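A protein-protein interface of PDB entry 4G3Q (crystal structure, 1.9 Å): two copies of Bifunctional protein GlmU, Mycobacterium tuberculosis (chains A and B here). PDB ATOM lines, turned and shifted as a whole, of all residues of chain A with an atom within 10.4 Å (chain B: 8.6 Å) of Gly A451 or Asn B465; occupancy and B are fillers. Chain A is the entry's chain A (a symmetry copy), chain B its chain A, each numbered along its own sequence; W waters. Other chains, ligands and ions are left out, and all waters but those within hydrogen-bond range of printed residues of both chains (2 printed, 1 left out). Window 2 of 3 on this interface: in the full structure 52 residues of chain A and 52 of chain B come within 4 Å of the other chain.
Gly A451 touches four residues of chain B.
Of chain A, only Gly A451 comes within 4 Å of Asn B465.
Ala A452 touches just one residue of chain B: Ile B463 (3.3 Å).
Glu B464 touches one residue of chain A.
Val B467 touches three residues of chain A.
Ser B480 touches three residues of chain A.
Of the printed residues of chain B, Leu A453 touches Asn B462, Ile B463 and Trp B466.
Printed residues of chain A within 4 Å of Ala B476: His A417 (3.3 Å), Gly A435 (3.5 Å) and Tyr A437 (3.95 Å).
Of the printed residues of chain B, Val A448 touches Asn B462 (3.9 Å).
Ile A432 touches none of the printed residues of chain B.
The nearest residue of chain A that does not touch Asn B465 is Ala A452 (4.2 Å).
The nearest printed residue of chain A that does not touch Arg B471 is Gly A435 (7.3 Å).
No position is printed for both chains.
Of the 25 pairs that touch across the chains among the printed residues, none has its exchanged pair printed and touching as well.
Of the 21 printed residues of chain A, 12 touch a printed residue of chain B.
Along chain A the printed residues that touch a printed residue of chain B span positions 417 to 454.
Of the 19 printed residues of chain B, 11 touch a printed residue of chain A.
Printed residues of chain B that touch a printed residue of chain A: Asn B462, Ile B463, Glu B464, Asn B465, Trp B466, Val B467, Arg B471, Ala B476, Ala B479, Ser B480 and Ala B483.
Hydrophobic or aromatic side chains of chain B within 4 Å of the printed part of chain A: Ile B463, Trp B466, Val B467, Ala B476, Ala B479 and Ala B483.
Along chain B the printed residues that touch a printed residue of chain A span positions 462 to 483.
Among the printed residues, no Asp or Glu carboxylate lies within 4 Å of a Lys or Arg side-chain nitrogen of the other chain.
Water W1 lies within hydrogen-bond range of the backbone carbonyl oxygen (O) of Ala B479 (2.7 Å), the side-chain carboxylate (OD2) of Asp A434 (2.9 Å) and the backbone NH (N) of Ala B483 (3.4 Å).
Water W2 lies within hydrogen-bond range of N of Asn B465 (2.7 Å), O of Pro A450 (2.9 Å), OE1 of Glu B464 (3.3 Å) and N of Ala A452 (3.3 Å).
The side-chain hydroxyl (OG) of Ser B480 is in hydrogen-bond range of the side-chain amide oxygen (OE1) of Gln B468 (2.9 Å).
The backbone NH (N) of Gly A435 sits at hydrogen-bond distance from the backbone carbonyl oxygen (O) of Ser A416, at 2.9 Å.
The backbone NH (N) of Gly A433 is in hydrogen-bond range of the backbone carbonyl oxygen (O) of Val A448.
The backbone NH (N) of Gly A451 is in hydrogen-bond range of the backbone carbonyl oxygen (O) of Asp A434 (3.1 Å).
The backbone carbonyl oxygen (O) of Ala A452 lies within hydrogen-bond range of the backbone NH (N) of Tyr A437 (3.0 Å).
The backbone carbonyl oxygen (O) of Tyr A437 is in hydrogen-bond range of the backbone NH (N) of Ala A454.
The side-chain amide nitrogen (ND2) of Asn B462 sits at hydrogen-bond distance from the backbone carbonyl oxygen (O) of Asp A447, 2.8 Å away.
N of Ile B463 sits at hydrogen-bond distance from O of Leu A453 (2.6 Å).
O of Gly A451 sits at hydrogen-bond distance from N of Trp B466.
The backbone carbonyl oxygen (O) of Gly A451 is in hydrogen-bond range of the backbone NH (N) of Val B467 (3.2 Å).
Among the printed residues, merely in contact across the chains: His A417 with Ala B476, His A417 with Ala B479, Asp A434 with Ala B479, Asp A434 with Ser B480, Asp A434 with Ala B483, Gly A435 with Val B467, Gly A435 with Ala B476, Tyr A437 with Trp B466, Tyr A437 with Val B467, Tyr A437 with Arg B471, Tyr A437 with Ala B476, Val A448 with Asn B462, Pro A449 with Asn B462, Pro A449 with Glu B464, Pro A450 with Ser B480, Gly A451 with Asn B465, Gly A451 with Ser B480, Ala A452 with Ile B463, Leu A453 with Asn B462, Leu A453 with Trp B466 and Ala A454 with Asn B462.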
ATOM      1  N   GLY A 415     -33.419   3.999 -16.977  1.00  0.00           N
ATOM      2  CA  GLY A 415     -33.042   3.695 -18.372  1.00  0.00           C
ATOM      3  C   GLY A 415     -33.438   2.310 -18.859  1.00  0.00           C
ATOM      4  O   GLY A 415     -34.274   1.616 -18.276  1.00  0.00           O
ATOM      5  N   SER A 416     -32.830   1.864 -19.942  1.00  0.00           N
ATOM      6  CA  SER A 416     -33.113   0.567 -20.513  1.00  0.00           C
ATOM      7  C   SER A 416     -32.113  -0.472 -20.089  1.00  0.00           C
ATOM      8  O   SER A 416     -30.955  -0.128 -19.762  1.00  0.00           O
ATOM      9  CB  SER A 416     -33.107   0.706 -22.064  1.00  0.00           C
ATOM     10  OG  SER A 416     -34.071   1.695 -22.448  1.00  0.00           O
ATOM     11  N   HIS A 417     -32.546  -1.728 -20.085  1.00  0.00           N
ATOM     12  CA  HIS A 417     -31.742  -2.905 -19.680  1.00  0.00           C
ATOM     13  C   HIS A 417     -31.274  -2.781 -18.226  1.00  0.00           C
ATOM     14  O   HIS A 417     -30.258  -3.369 -17.844  1.00  0.00           O
ATOM     15  CB  HIS A 417     -30.549  -3.113 -20.660  1.00  0.00           C
ATOM     16  CG  HIS A 417     -30.984  -3.233 -22.089  1.00  0.00           C
ATOM     17  ND1 HIS A 417     -31.401  -4.429 -22.621  1.00  0.00           N
ATOM     18  CD2 HIS A 417     -31.108  -2.312 -23.076  1.00  0.00           C
ATOM     19  CE1 HIS A 417     -31.767  -4.244 -23.880  1.00  0.00           C
ATOM     20  NE2 HIS A 417     -31.596  -2.972 -24.178  1.00  0.00           N
ATOM     21  N   VAL A 418     -31.984  -1.981 -17.429  1.00  0.00           N
ATOM     22  CA  VAL A 418     -31.653  -1.928 -16.006  1.00  0.00           C
ATOM     23  C   VAL A 418     -32.218  -3.127 -15.201  1.00  0.00           C
ATOM     24  O   VAL A 418     -33.273  -3.677 -15.569  1.00  0.00           O
ATOM     25  CB  VAL A 418     -31.801  -0.516 -15.346  1.00  0.00           C
ATOM     26  CG1 VAL A 418     -31.861   0.720 -16.273  1.00  0.00           C
ATOM     27  CG2 VAL A 418     -32.476  -0.456 -14.013  1.00  0.00           C
ATOM     28  N   ARG A 419     -31.508  -3.571 -14.158  1.00  0.00           N
ATOM     29  CA  ARG A 419     -32.066  -4.644 -13.325  1.00  0.00           C
ATOM     30  C   ARG A 419     -32.024  -4.158 -11.891  1.00  0.00           C
ATOM     31  O   ARG A 419     -30.936  -4.057 -11.259  1.00  0.00           O
ATOM     32  CB  ARG A 419     -31.291  -5.960 -13.468  1.00  0.00           C
ATOM     33  CG  ARG A 419     -31.256  -6.569 -14.918  1.00  0.00           C
ATOM     34  CD  ARG A 419     -32.337  -7.638 -15.032  1.00  0.00           C
ATOM     35  NE  ARG A 419     -32.383  -8.353 -16.316  1.00  0.00           N
ATOM     36  CZ  ARG A 419     -32.825  -7.864 -17.480  1.00  0.00           C
ATOM     37  NH1 ARG A 419     -32.782  -8.642 -18.570  1.00  0.00           N
ATOM     38  NH2 ARG A 419     -33.289  -6.617 -17.595  1.00  0.00           N
ATOM     39  N   THR A 431     -32.154   9.658 -11.322  1.00  0.00           N
ATOM     40  CA  THR A 431     -32.012   9.071 -12.650  1.00  0.00           C
ATOM     41  C   THR A 431     -31.166   7.818 -12.544  1.00  0.00           C
ATOM     42  O   THR A 431     -30.101   7.851 -11.934  1.00  0.00           O
ATOM     43  CB  THR A 431     -31.365  10.098 -13.612  1.00  0.00           C
ATOM     44  OG1 THR A 431     -32.196  11.266 -13.616  1.00  0.00           O
ATOM     45  CG2 THR A 431     -31.209   9.537 -15.003  1.00  0.00           C
ATOM     46  N   ILE A 432     -31.645   6.708 -13.090  1.00  0.00           N
ATOM     47  CA  ILE A 432     -30.878   5.473 -13.100  1.00  0.00           C
ATOM     48  C   ILE A 432     -30.472   5.214 -14.527  1.00  0.00           C
ATOM     49  O   ILE A 432     -31.326   5.009 -15.394  1.00  0.00           O
ATOM     50  CB  ILE A 432     -31.742   4.282 -12.678  1.00  0.00           C
ATOM     51  CG1 ILE A 432     -32.451   4.568 -11.356  1.00  0.00           C
ATOM     52  CG2 ILE A 432     -30.912   2.954 -12.661  1.00  0.00           C
ATOM     53  CD1 ILE A 432     -31.593   4.432 -10.152  1.00  0.00           C
ATOM     54  N   GLY A 433     -29.152   5.222 -14.804  1.00  0.00           N
ATOM     55  CA  GLY A 433     -28.708   5.009 -16.168  1.00  0.00           C
ATOM     56  C   GLY A 433     -28.886   3.643 -16.784  1.00  0.00           C
ATOM     57  O   GLY A 433     -29.040   2.606 -16.099  1.00  0.00           O
ATOM     58  N   ASP A 434     -28.733   3.595 -18.112  1.00  0.00           N
ATOM     59  CA  ASP A 434     -28.932   2.377 -18.827  1.00  0.00           C
ATOM     60  C   ASP A 434     -28.034   1.262 -18.286  1.00  0.00           C
ATOM     61  O   ASP A 434     -26.837   1.458 -18.024  1.00  0.00           O
ATOM     62  CB  ASP A 434     -28.615   2.531 -20.334  1.00  0.00           C
ATOM     63  CG  ASP A 434     -29.625   3.416 -21.074  1.00  0.00           C
ATOM     64  OD1 ASP A 434     -30.768   3.657 -20.561  1.00  0.00           O
ATOM     65  OD2 ASP A 434     -29.261   3.885 -22.178  1.00  0.00           O
ATOM     66  N   GLY A 435     -28.586   0.076 -18.186  1.00  0.00           N
ATOM     67  CA  GLY A 435     -27.815  -1.110 -17.774  1.00  0.00           C
ATOM     68  C   GLY A 435     -27.338  -1.129 -16.328  1.00  0.00           C
ATOM     69  O   GLY A 435     -26.600  -2.066 -15.941  1.00  0.00           O
ATOM     70  N   ALA A 436     -27.675  -0.104 -15.536  1.00  0.00           N
ATOM     71  CA  ALA A 436     -27.362  -0.111 -14.085  1.00  0.00           C
ATOM     72  C   ALA A 436     -28.126  -1.217 -13.323  1.00  0.00           C
ATOM     73  O   ALA A 436     -29.171  -1.725 -13.782  1.00  0.00           O
ATOM     74  CB  ALA A 436     -27.595   1.272 -13.440  1.00  0.00           C
ATOM     75  N   TYR A 437     -27.605  -1.568 -12.154  1.00  0.00           N
ATOM     76  CA  TYR A 437     -28.222  -2.537 -11.213  1.00  0.00           C
ATOM     77  C   TYR A 437     -28.374  -1.840  -9.874  1.00  0.00           C
ATOM     78  O   TYR A 437     -27.629  -0.857  -9.564  1.00  0.00           O
ATOM     79  CB  TYR A 437     -27.287  -3.750 -10.952  1.00  0.00           C
ATOM     80  CG  TYR A 437     -27.409  -4.961 -11.882  1.00  0.00           C
ATOM     81  CD1 TYR A 437     -27.561  -6.236 -11.358  1.00  0.00           C
ATOM     82  CD2 TYR A 437     -27.365  -4.824 -13.281  1.00  0.00           C
ATOM     83  CE1 TYR A 437     -27.680  -7.369 -12.210  1.00  0.00           C
ATOM     84  CE2 TYR A 437     -27.446  -5.916 -14.110  1.00  0.00           C
ATOM     85  CZ  TYR A 437     -27.600  -7.186 -13.573  1.00  0.00           C
ATOM     86  OH  TYR A 437     -27.705  -8.276 -14.406  1.00  0.00           O
ATOM     87  N   THR A 438     -29.348  -2.300  -9.070  1.00  0.00           N
ATOM     88  CA  THR A 438     -29.298  -1.948  -7.630  1.00  0.00           C
ATOM     89  C   THR A 438     -29.293  -3.223  -6.803  1.00  0.00           C
ATOM     90  O   THR A 438     -29.843  -4.225  -7.239  1.00  0.00           O
ATOM     91  CB  THR A 438     -30.478  -1.034  -7.182  1.00  0.00           C
ATOM     92  OG1 THR A 438     -31.697  -1.769  -7.227  1.00  0.00           O
ATOM     93  CG2 THR A 438     -30.642   0.108  -8.114  1.00  0.00           C
ATOM     94  N   ASP A 447     -28.568   9.900  -8.235  1.00  0.00           N
ATOM     95  CA  ASP A 447     -28.301   9.315  -9.553  1.00  0.00           C
ATOM     96  C   ASP A 447     -27.337   8.124  -9.544  1.00  0.00           C
ATOM     97  O   ASP A 447     -26.423   8.055  -8.714  1.00  0.00           O
ATOM     98  CB  ASP A 447     -27.819  10.418 -10.510  1.00  0.00           C
ATOM     99  CG  ASP A 447     -28.905  11.522 -10.740  1.00  0.00           C
ATOM    100  OD1 ASP A 447     -30.073  11.372 -10.294  1.00  0.00           O
ATOM    101  OD2 ASP A 447     -28.579  12.567 -11.353  1.00  0.00           O
ATOM    102  N   VAL A 448     -27.577   7.181 -10.445  1.00  0.00           N
ATOM    103  CA  VAL A 448     -26.808   5.953 -10.613  1.00  0.00           C
ATOM    104  C   VAL A 448     -26.361   5.972 -12.089  1.00  0.00           C
ATOM    105  O   VAL A 448     -27.197   5.870 -13.041  1.00  0.00           O
ATOM    106  CB  VAL A 448     -27.677   4.693 -10.324  1.00  0.00           C
ATOM    107  CG1 VAL A 448     -26.890   3.362 -10.529  1.00  0.00           C
ATOM    108  CG2 VAL A 448     -28.213   4.733  -8.923  1.00  0.00           C
ATOM    109  N   PRO A 449     -25.036   6.138 -12.320  1.00  0.00           N
ATOM    110  CA  PRO A 449     -24.539   6.039 -13.683  1.00  0.00           C
ATOM    111  C   PRO A 449     -24.884   4.763 -14.436  1.00  0.00           C
ATOM    112  O   PRO A 449     -25.062   3.672 -13.852  1.00  0.00           O
ATOM    113  CB  PRO A 449     -22.998   6.070 -13.518  1.00  0.00           C
ATOM    114  CG  PRO A 449     -22.789   6.900 -12.363  1.00  0.00           C
ATOM    115  CD  PRO A 449     -23.949   6.452 -11.375  1.00  0.00           C
ATOM    116  N   PRO A 450     -24.881   4.848 -15.774  1.00  0.00           N
ATOM    117  CA  PRO A 450     -25.026   3.614 -16.583  1.00  0.00           C
ATOM    118  C   PRO A 450     -24.027   2.558 -16.156  1.00  0.00           C
ATOM    119  O   PRO A 450     -22.832   2.881 -15.883  1.00  0.00           O
ATOM    120  CB  PRO A 450     -24.736   4.111 -18.037  1.00  0.00           C
ATOM    121  CG  PRO A 450     -25.058   5.574 -18.011  1.00  0.00           C
ATOM    122  CD  PRO A 450     -24.686   6.058 -16.605  1.00  0.00           C
ATOM    123  N   GLY A 451     -24.510   1.339 -16.000  1.00  0.00           N
ATOM    124  CA  GLY A 451     -23.680   0.195 -15.661  1.00  0.00           C
ATOM    125  C   GLY A 451     -23.073   0.202 -14.257  1.00  0.00           C
ATOM    126  O   GLY A 451     -22.195  -0.599 -14.006  1.00  0.00           O
ATOM    127  N   ALA A 452     -23.461   1.138 -13.398  1.00  0.00           N
ATOM    128  CA  ALA A 452     -23.059   1.143 -11.979  1.00  0.00           C
ATOM    129  C   ALA A 452     -23.949   0.181 -11.201  1.00  0.00           C
ATOM    130  O   ALA A 452     -25.047  -0.179 -11.674  1.00  0.00           O
ATOM    131  CB  ALA A 452     -23.167   2.606 -11.368  1.00  0.00           C
ATOM    132  N   LEU A 453     -23.434  -0.321 -10.085  1.00  0.00           N
ATOM    133  CA  LEU A 453     -24.271  -1.059  -9.127  1.00  0.00           C
ATOM    134  C   LEU A 453     -24.437  -0.111  -7.914  1.00  0.00           C
ATOM    135  O   LEU A 453     -23.455   0.398  -7.359  1.00  0.00           O
ATOM    136  CB  LEU A 453     -23.693  -2.436  -8.777  1.00  0.00           C
ATOM    137  CG  LEU A 453     -24.259  -3.079  -7.483  1.00  0.00           C
ATOM    138  CD1 LEU A 453     -25.746  -3.488  -7.604  1.00  0.00           C
ATOM    139  CD2 LEU A 453     -23.434  -4.333  -6.907  1.00  0.00           C
ATOM    140  N   ALA A 454     -25.694   0.241  -7.585  1.00  0.00           N
ATOM    141  CA  ALA A 454     -25.977   1.065  -6.410  1.00  0.00           C
ATOM    142  C   ALA A 454     -26.405   0.119  -5.256  1.00  0.00           C
ATOM    143  O   ALA A 454     -27.282  -0.761  -5.425  1.00  0.00           O
ATOM    144  CB  ALA A 454     -27.082   2.113  -6.711  1.00  0.00           C
ATOM    145  N   ASN B 462     -22.431   4.084  -5.015  1.00  0.00           N
ATOM    146  CA  ASN B 462     -22.429   3.608  -6.401  1.00  0.00           C
ATOM    147  C   ASN B 462     -21.123   2.902  -6.699  1.00  0.00           C
ATOM    148  O   ASN B 462     -20.080   3.477  -6.415  1.00  0.00           O
ATOM    149  CB  ASN B 462     -22.596   4.766  -7.407  1.00  0.00           C
ATOM    150  CG  ASN B 462     -24.011   5.366  -7.349  1.00  0.00           C
ATOM    151  OD1 ASN B 462     -24.934   4.698  -6.853  1.00  0.00           O
ATOM    152  ND2 ASN B 462     -24.176   6.607  -7.791  1.00  0.00           N
ATOM    153  N   ILE B 463     -21.176   1.690  -7.244  1.00  0.00           N
ATOM    154  CA  ILE B 463     -19.958   0.951  -7.700  1.00  0.00           C
ATOM    155  C   ILE B 463     -19.858   1.057  -9.234  1.00  0.00           C
ATOM    156  O   ILE B 463     -20.535   0.321  -9.978  1.00  0.00           O
ATOM    157  CB  ILE B 463     -19.986  -0.489  -7.244  1.00  0.00           C
ATOM    158  CG1 ILE B 463     -20.247  -0.543  -5.724  1.00  0.00           C
ATOM    159  CG2 ILE B 463     -18.696  -1.298  -7.689  1.00  0.00           C
ATOM    160  CD1 ILE B 463     -20.743  -1.875  -5.219  1.00  0.00           C
ATOM    161  N   GLU B 464     -18.992   1.948  -9.685  1.00  0.00           N
ATOM    162  CA  GLU B 464     -18.888   2.234 -11.123  1.00  0.00           C
ATOM    163  C   GLU B 464     -18.381   1.044 -11.905  1.00  0.00           C
ATOM    164  O   GLU B 464     -17.469   0.309 -11.453  1.00  0.00           O
ATOM    165  CB  GLU B 464     -17.970   3.424 -11.402  1.00  0.00           C
ATOM    166  CG  GLU B 464     -18.265   4.652 -10.587  1.00  0.00           C
ATOM    167  CD  GLU B 464     -18.947   5.733 -11.389  1.00  0.00           C
ATOM    168  OE1 GLU B 464     -19.737   5.394 -12.325  1.00  0.00           O
ATOM    169  OE2 GLU B 464     -18.679   6.917 -11.086  1.00  0.00           O
ATOM    170  N   ASN B 465     -18.976   0.850 -13.088  1.00  0.00           N
ATOM    171  CA  ASN B 465     -18.626  -0.236 -13.990  1.00  0.00           C
ATOM    172  C   ASN B 465     -18.753  -1.639 -13.449  1.00  0.00           C
ATOM    173  O   ASN B 465     -18.138  -2.561 -13.999  1.00  0.00           O
ATOM    174  CB  ASN B 465     -17.216   0.007 -14.593  1.00  0.00           C
ATOM    175  CG  ASN B 465     -17.161   1.310 -15.421  1.00  0.00           C
ATOM    176  OD1 ASN B 465     -17.706   1.357 -16.520  1.00  0.00           O
ATOM    177  ND2 ASN B 465     -16.583   2.379 -14.854  1.00  0.00           N
ATOM    178  N   TRP B 466     -19.574  -1.832 -12.402  1.00  0.00           N
ATOM    179  CA  TRP B 466     -19.775  -3.147 -11.818  1.00  0.00           C
ATOM    180  C   TRP B 466     -20.339  -4.115 -12.860  1.00  0.00           C
ATOM    181  O   TRP B 466     -19.890  -5.285 -12.949  1.00  0.00           O
ATOM    182  CB  TRP B 466     -20.676  -3.062 -10.564  1.00  0.00           C
ATOM    183  CG  TRP B 466     -20.907  -4.342  -9.899  1.00  0.00           C
ATOM    184  CD1 TRP B 466     -20.174  -4.894  -8.869  1.00  0.00           C
ATOM    185  CD2 TRP B 466     -21.938  -5.273 -10.206  1.00  0.00           C
ATOM    186  NE1 TRP B 466     -20.705  -6.128  -8.524  1.00  0.00           N
ATOM    187  CE2 TRP B 466     -21.767  -6.392  -9.352  1.00  0.00           C
ATOM    188  CE3 TRP B 466     -22.973  -5.294 -11.165  1.00  0.00           C
ATOM    189  CZ2 TRP B 466     -22.641  -7.516  -9.390  1.00  0.00           C
ATOM    190  CZ3 TRP B 466     -23.817  -6.372 -11.206  1.00  0.00           C
ATOM    191  CH2 TRP B 466     -23.660  -7.483 -10.327  1.00  0.00           C
ATOM    192  N   VAL B 467     -21.323  -3.624 -13.635  1.00  0.00           N
ATOM    193  CA  VAL B 467     -21.978  -4.462 -14.627  1.00  0.00           C
ATOM    194  C   VAL B 467     -21.010  -4.994 -15.734  1.00  0.00           C
ATOM    195  O   VAL B 467     -21.076  -6.179 -16.104  1.00  0.00           O
ATOM    196  CB  VAL B 467     -23.276  -3.736 -15.232  1.00  0.00           C
ATOM    197  CG1 VAL B 467     -23.997  -4.647 -16.164  1.00  0.00           C
ATOM    198  CG2 VAL B 467     -24.241  -3.391 -14.078  1.00  0.00           C
ATOM    199  N   GLN B 468     -20.126  -4.139 -16.244  1.00  0.00           N
ATOM    200  CA  GLN B 468     -19.110  -4.561 -17.205  1.00  0.00           C
ATOM    201  C   GLN B 468     -18.241  -5.654 -16.589  1.00  0.00           C
ATOM    202  O   GLN B 468     -17.929  -6.639 -17.278  1.00  0.00           O
ATOM    203  CB  GLN B 468     -18.216  -3.410 -17.691  1.00  0.00           C
ATOM    204  CG  GLN B 468     -18.930  -2.104 -18.021  1.00  0.00           C
ATOM    205  CD  GLN B 468     -19.170  -1.855 -19.497  1.00  0.00           C
ATOM    206  OE1 GLN B 468     -20.327  -1.763 -19.957  1.00  0.00           O
ATOM    207  NE2 GLN B 468     -18.072  -1.731 -20.260  1.00  0.00           N
ATOM    208  N   ARG B 469     -17.905  -5.538 -15.298  1.00  0.00           N
ATOM    209  CA  ARG B 469     -17.025  -6.545 -14.655  1.00  0.00           C
ATOM    210  C   ARG B 469     -17.706  -7.856 -14.324  1.00  0.00           C
ATOM    211  O   ARG B 469     -17.136  -8.907 -14.580  1.00  0.00           O
ATOM    212  CB  ARG B 469     -16.434  -6.060 -13.340  1.00  0.00           C
ATOM    213  CG  ARG B 469     -15.369  -5.004 -13.388  1.00  0.00           C
ATOM    214  CD  ARG B 469     -15.178  -4.613 -11.884  1.00  0.00           C
ATOM    215  NE  ARG B 469     -14.947  -3.213 -11.860  1.00  0.00           N
ATOM    216  CZ  ARG B 469     -15.510  -2.310 -11.095  1.00  0.00           C
ATOM    217  NH1 ARG B 469     -16.358  -2.603 -10.122  1.00  0.00           N
ATOM    218  NH2 ARG B 469     -15.132  -1.064 -11.315  1.00  0.00           N
ATOM    219  N   LYS B 470     -18.903  -7.786 -13.721  1.00  0.00           N
ATOM    220  CA  LYS B 470     -19.617  -8.966 -13.226  1.00  0.00           C
ATOM    221  C   LYS B 470     -20.745  -9.519 -14.062  1.00  0.00           C
ATOM    222  O   LYS B 470     -21.207 -10.640 -13.801  1.00  0.00           O
ATOM    223  CB  LYS B 470     -20.134  -8.757 -11.797  1.00  0.00           C
ATOM    224  CG  LYS B 470     -19.093  -8.197 -10.861  1.00  0.00           C
ATOM    225  CD  LYS B 470     -17.895  -9.175 -10.681  1.00  0.00           C
ATOM    226  CE  LYS B 470     -18.326 -10.601 -10.384  1.00  0.00           C
ATOM    227  NZ  LYS B 470     -19.160 -10.777  -9.143  1.00  0.00           N
ATOM    228  N   ARG B 471     -21.200  -8.761 -15.055  1.00  0.00           N
ATOM    229  CA  ARG B 471     -22.194  -9.317 -16.037  1.00  0.00           C
ATOM    230  C   ARG B 471     -21.659  -9.065 -17.452  1.00  0.00           C
ATOM    231  O   ARG B 471     -22.362  -8.449 -18.284  1.00  0.00           O
ATOM    232  CB  ARG B 471     -23.590  -8.669 -15.860  1.00  0.00           C
ATOM    233  CG  ARG B 471     -24.217  -8.859 -14.454  1.00  0.00           C
ATOM    234  CD  ARG B 471     -24.605 -10.312 -14.187  1.00  0.00           C
ATOM    235  NE  ARG B 471     -25.262 -10.485 -12.888  1.00  0.00           N
ATOM    236  CZ  ARG B 471     -24.641 -10.757 -11.727  1.00  0.00           C
ATOM    237  NH1 ARG B 471     -23.324 -10.906 -11.666  1.00  0.00           N
ATOM    238  NH2 ARG B 471     -25.361 -10.871 -10.612  1.00  0.00           N
ATOM    239  N   PRO B 472     -20.396  -9.484 -17.731  1.00  0.00           N
ATOM    240  CA  PRO B 472     -19.754  -9.143 -19.026  1.00  0.00           C
ATOM    241  C   PRO B 472     -20.585  -9.675 -20.226  1.00  0.00           C
ATOM    242  O   PRO B 472     -21.073 -10.813 -20.166  1.00  0.00           O
ATOM    243  CB  PRO B 472     -18.391  -9.886 -18.932  1.00  0.00           C
ATOM    244  CG  PRO B 472     -18.676 -11.054 -18.068  1.00  0.00           C
ATOM    245  CD  PRO B 472     -19.588 -10.481 -16.987  1.00  0.00           C
ATOM    246  N   ALA B 476     -27.425  -5.821 -20.205  1.00  0.00           N
ATOM    247  CA  ALA B 476     -27.112  -4.602 -19.395  1.00  0.00           C
ATOM    248  C   ALA B 476     -25.675  -4.029 -19.639  1.00  0.00           C
ATOM    249  O   ALA B 476     -25.494  -2.793 -19.718  1.00  0.00           O
ATOM    250  CB  ALA B 476     -27.346  -4.844 -17.914  1.00  0.00           C
ATOM    251  N   ALA B 477     -24.676  -4.913 -19.741  1.00  0.00           N
ATOM    252  CA  ALA B 477     -23.305  -4.471 -20.054  1.00  0.00           C
ATOM    253  C   ALA B 477     -23.217  -3.759 -21.407  1.00  0.00           C
ATOM    254  O   ALA B 477     -22.651  -2.651 -21.495  1.00  0.00           O
ATOM    255  CB  ALA B 477     -22.256  -5.645 -19.937  1.00  0.00           C
ATOM    256  N   GLN B 478     -23.796  -4.366 -22.452  1.00  0.00           N
ATOM    257  CA  GLN B 478     -23.834  -3.725 -23.800  1.00  0.00           C
ATOM    258  C   GLN B 478     -24.525  -2.358 -23.741  1.00  0.00           C
ATOM    259  O   GLN B 478     -24.071  -1.382 -24.394  1.00  0.00           O
ATOM    260  CB  GLN B 478     -24.514  -4.660 -24.828  1.00  0.00           C
ATOM    261  CG  GLN B 478     -23.896  -6.081 -24.845  1.00  0.00           C
ATOM    262  CD  GLN B 478     -24.753  -7.116 -25.612  1.00  0.00           C
ATOM    263  OE1 GLN B 478     -25.249  -8.112 -25.044  1.00  0.00           O
ATOM    264  NE2 GLN B 478     -24.939  -6.868 -26.906  1.00  0.00           N
ATOM    265  N   ALA B 479     -25.603  -2.266 -22.934  1.00  0.00           N
ATOM    266  CA  ALA B 479     -26.377  -1.009 -22.808  1.00  0.00           C
ATOM    267  C   ALA B 479     -25.582   0.107 -22.109  1.00  0.00           C
ATOM    268  O   ALA B 479     -25.686   1.251 -22.516  1.00  0.00           O
ATOM    269  CB  ALA B 479     -27.764  -1.250 -22.069  1.00  0.00           C
ATOM    270  N   SER B 480     -24.822  -0.213 -21.043  1.00  0.00           N
ATOM    271  CA  SER B 480     -24.020   0.820 -20.360  1.00  0.00           C
ATOM    272  C   SER B 480     -22.863   1.270 -21.265  1.00  0.00           C
ATOM    273  O   SER B 480     -22.548   2.463 -21.298  1.00  0.00           O
ATOM    274  CB  SER B 480     -23.449   0.342 -19.034  1.00  0.00           C
ATOM    275  OG  SER B 480     -23.027  -0.989 -19.163  1.00  0.00           O
ATOM    276  N   LYS B 481     -22.260   0.309 -21.976  1.00  0.00           N
ATOM    277  CA  LYS B 481     -21.325   0.563 -23.103  1.00  0.00           C
ATOM    278  C   LYS B 481     -21.952   1.538 -24.149  1.00  0.00           C
ATOM    279  O   LYS B 481     -21.406   2.621 -24.378  1.00  0.00           O
ATOM    280  CB  LYS B 481     -20.890  -0.778 -23.737  1.00  0.00           C
ATOM    281  CG  LYS B 481     -20.068  -0.690 -25.042  1.00  0.00           C
ATOM    282  CD  LYS B 481     -20.333  -1.913 -25.982  1.00  0.00           C
ATOM    283  CE  LYS B 481     -19.198  -2.952 -25.955  1.00  0.00           C
ATOM    284  NZ  LYS B 481     -19.125  -3.746 -24.673  1.00  0.00           N
ATOM    285  N   ALA B 483     -24.517   3.575 -23.915  1.00  0.00           N
ATOM    286  CA  ALA B 483     -24.829   4.894 -23.320  1.00  0.00           C
ATOM    287  C   ALA B 483     -23.561   5.735 -23.094  1.00  0.00           C
ATOM    288  O   ALA B 483     -23.588   6.967 -23.209  1.00  0.00           O
ATOM    289  CB  ALA B 483     -25.616   4.738 -22.008  1.00  0.00           C
ATOM    290  N   SER B 484     -22.469   5.042 -22.758  1.00  0.00           N
ATOM    291  CA  SER B 484     -21.109   5.596 -22.659  1.00  0.00           C
ATOM    292  C   SER B 484     -20.648   6.320 -23.947  1.00  0.00           C
ATOM    293  O   SER B 484     -20.154   7.454 -23.876  1.00  0.00           O
ATOM    294  CB  SER B 484     -20.141   4.457 -22.268  1.00  0.00           C
ATOM    295  OG  SER B 484     -18.776   4.819 -22.364  1.00  0.00           O
HETATM  296  O   HOH W   1     -27.668   2.228 -23.989  1.00  0.00           O
HETATM  297  O   HOH W   2     -20.675   2.770 -14.013  1.00  0.00           O
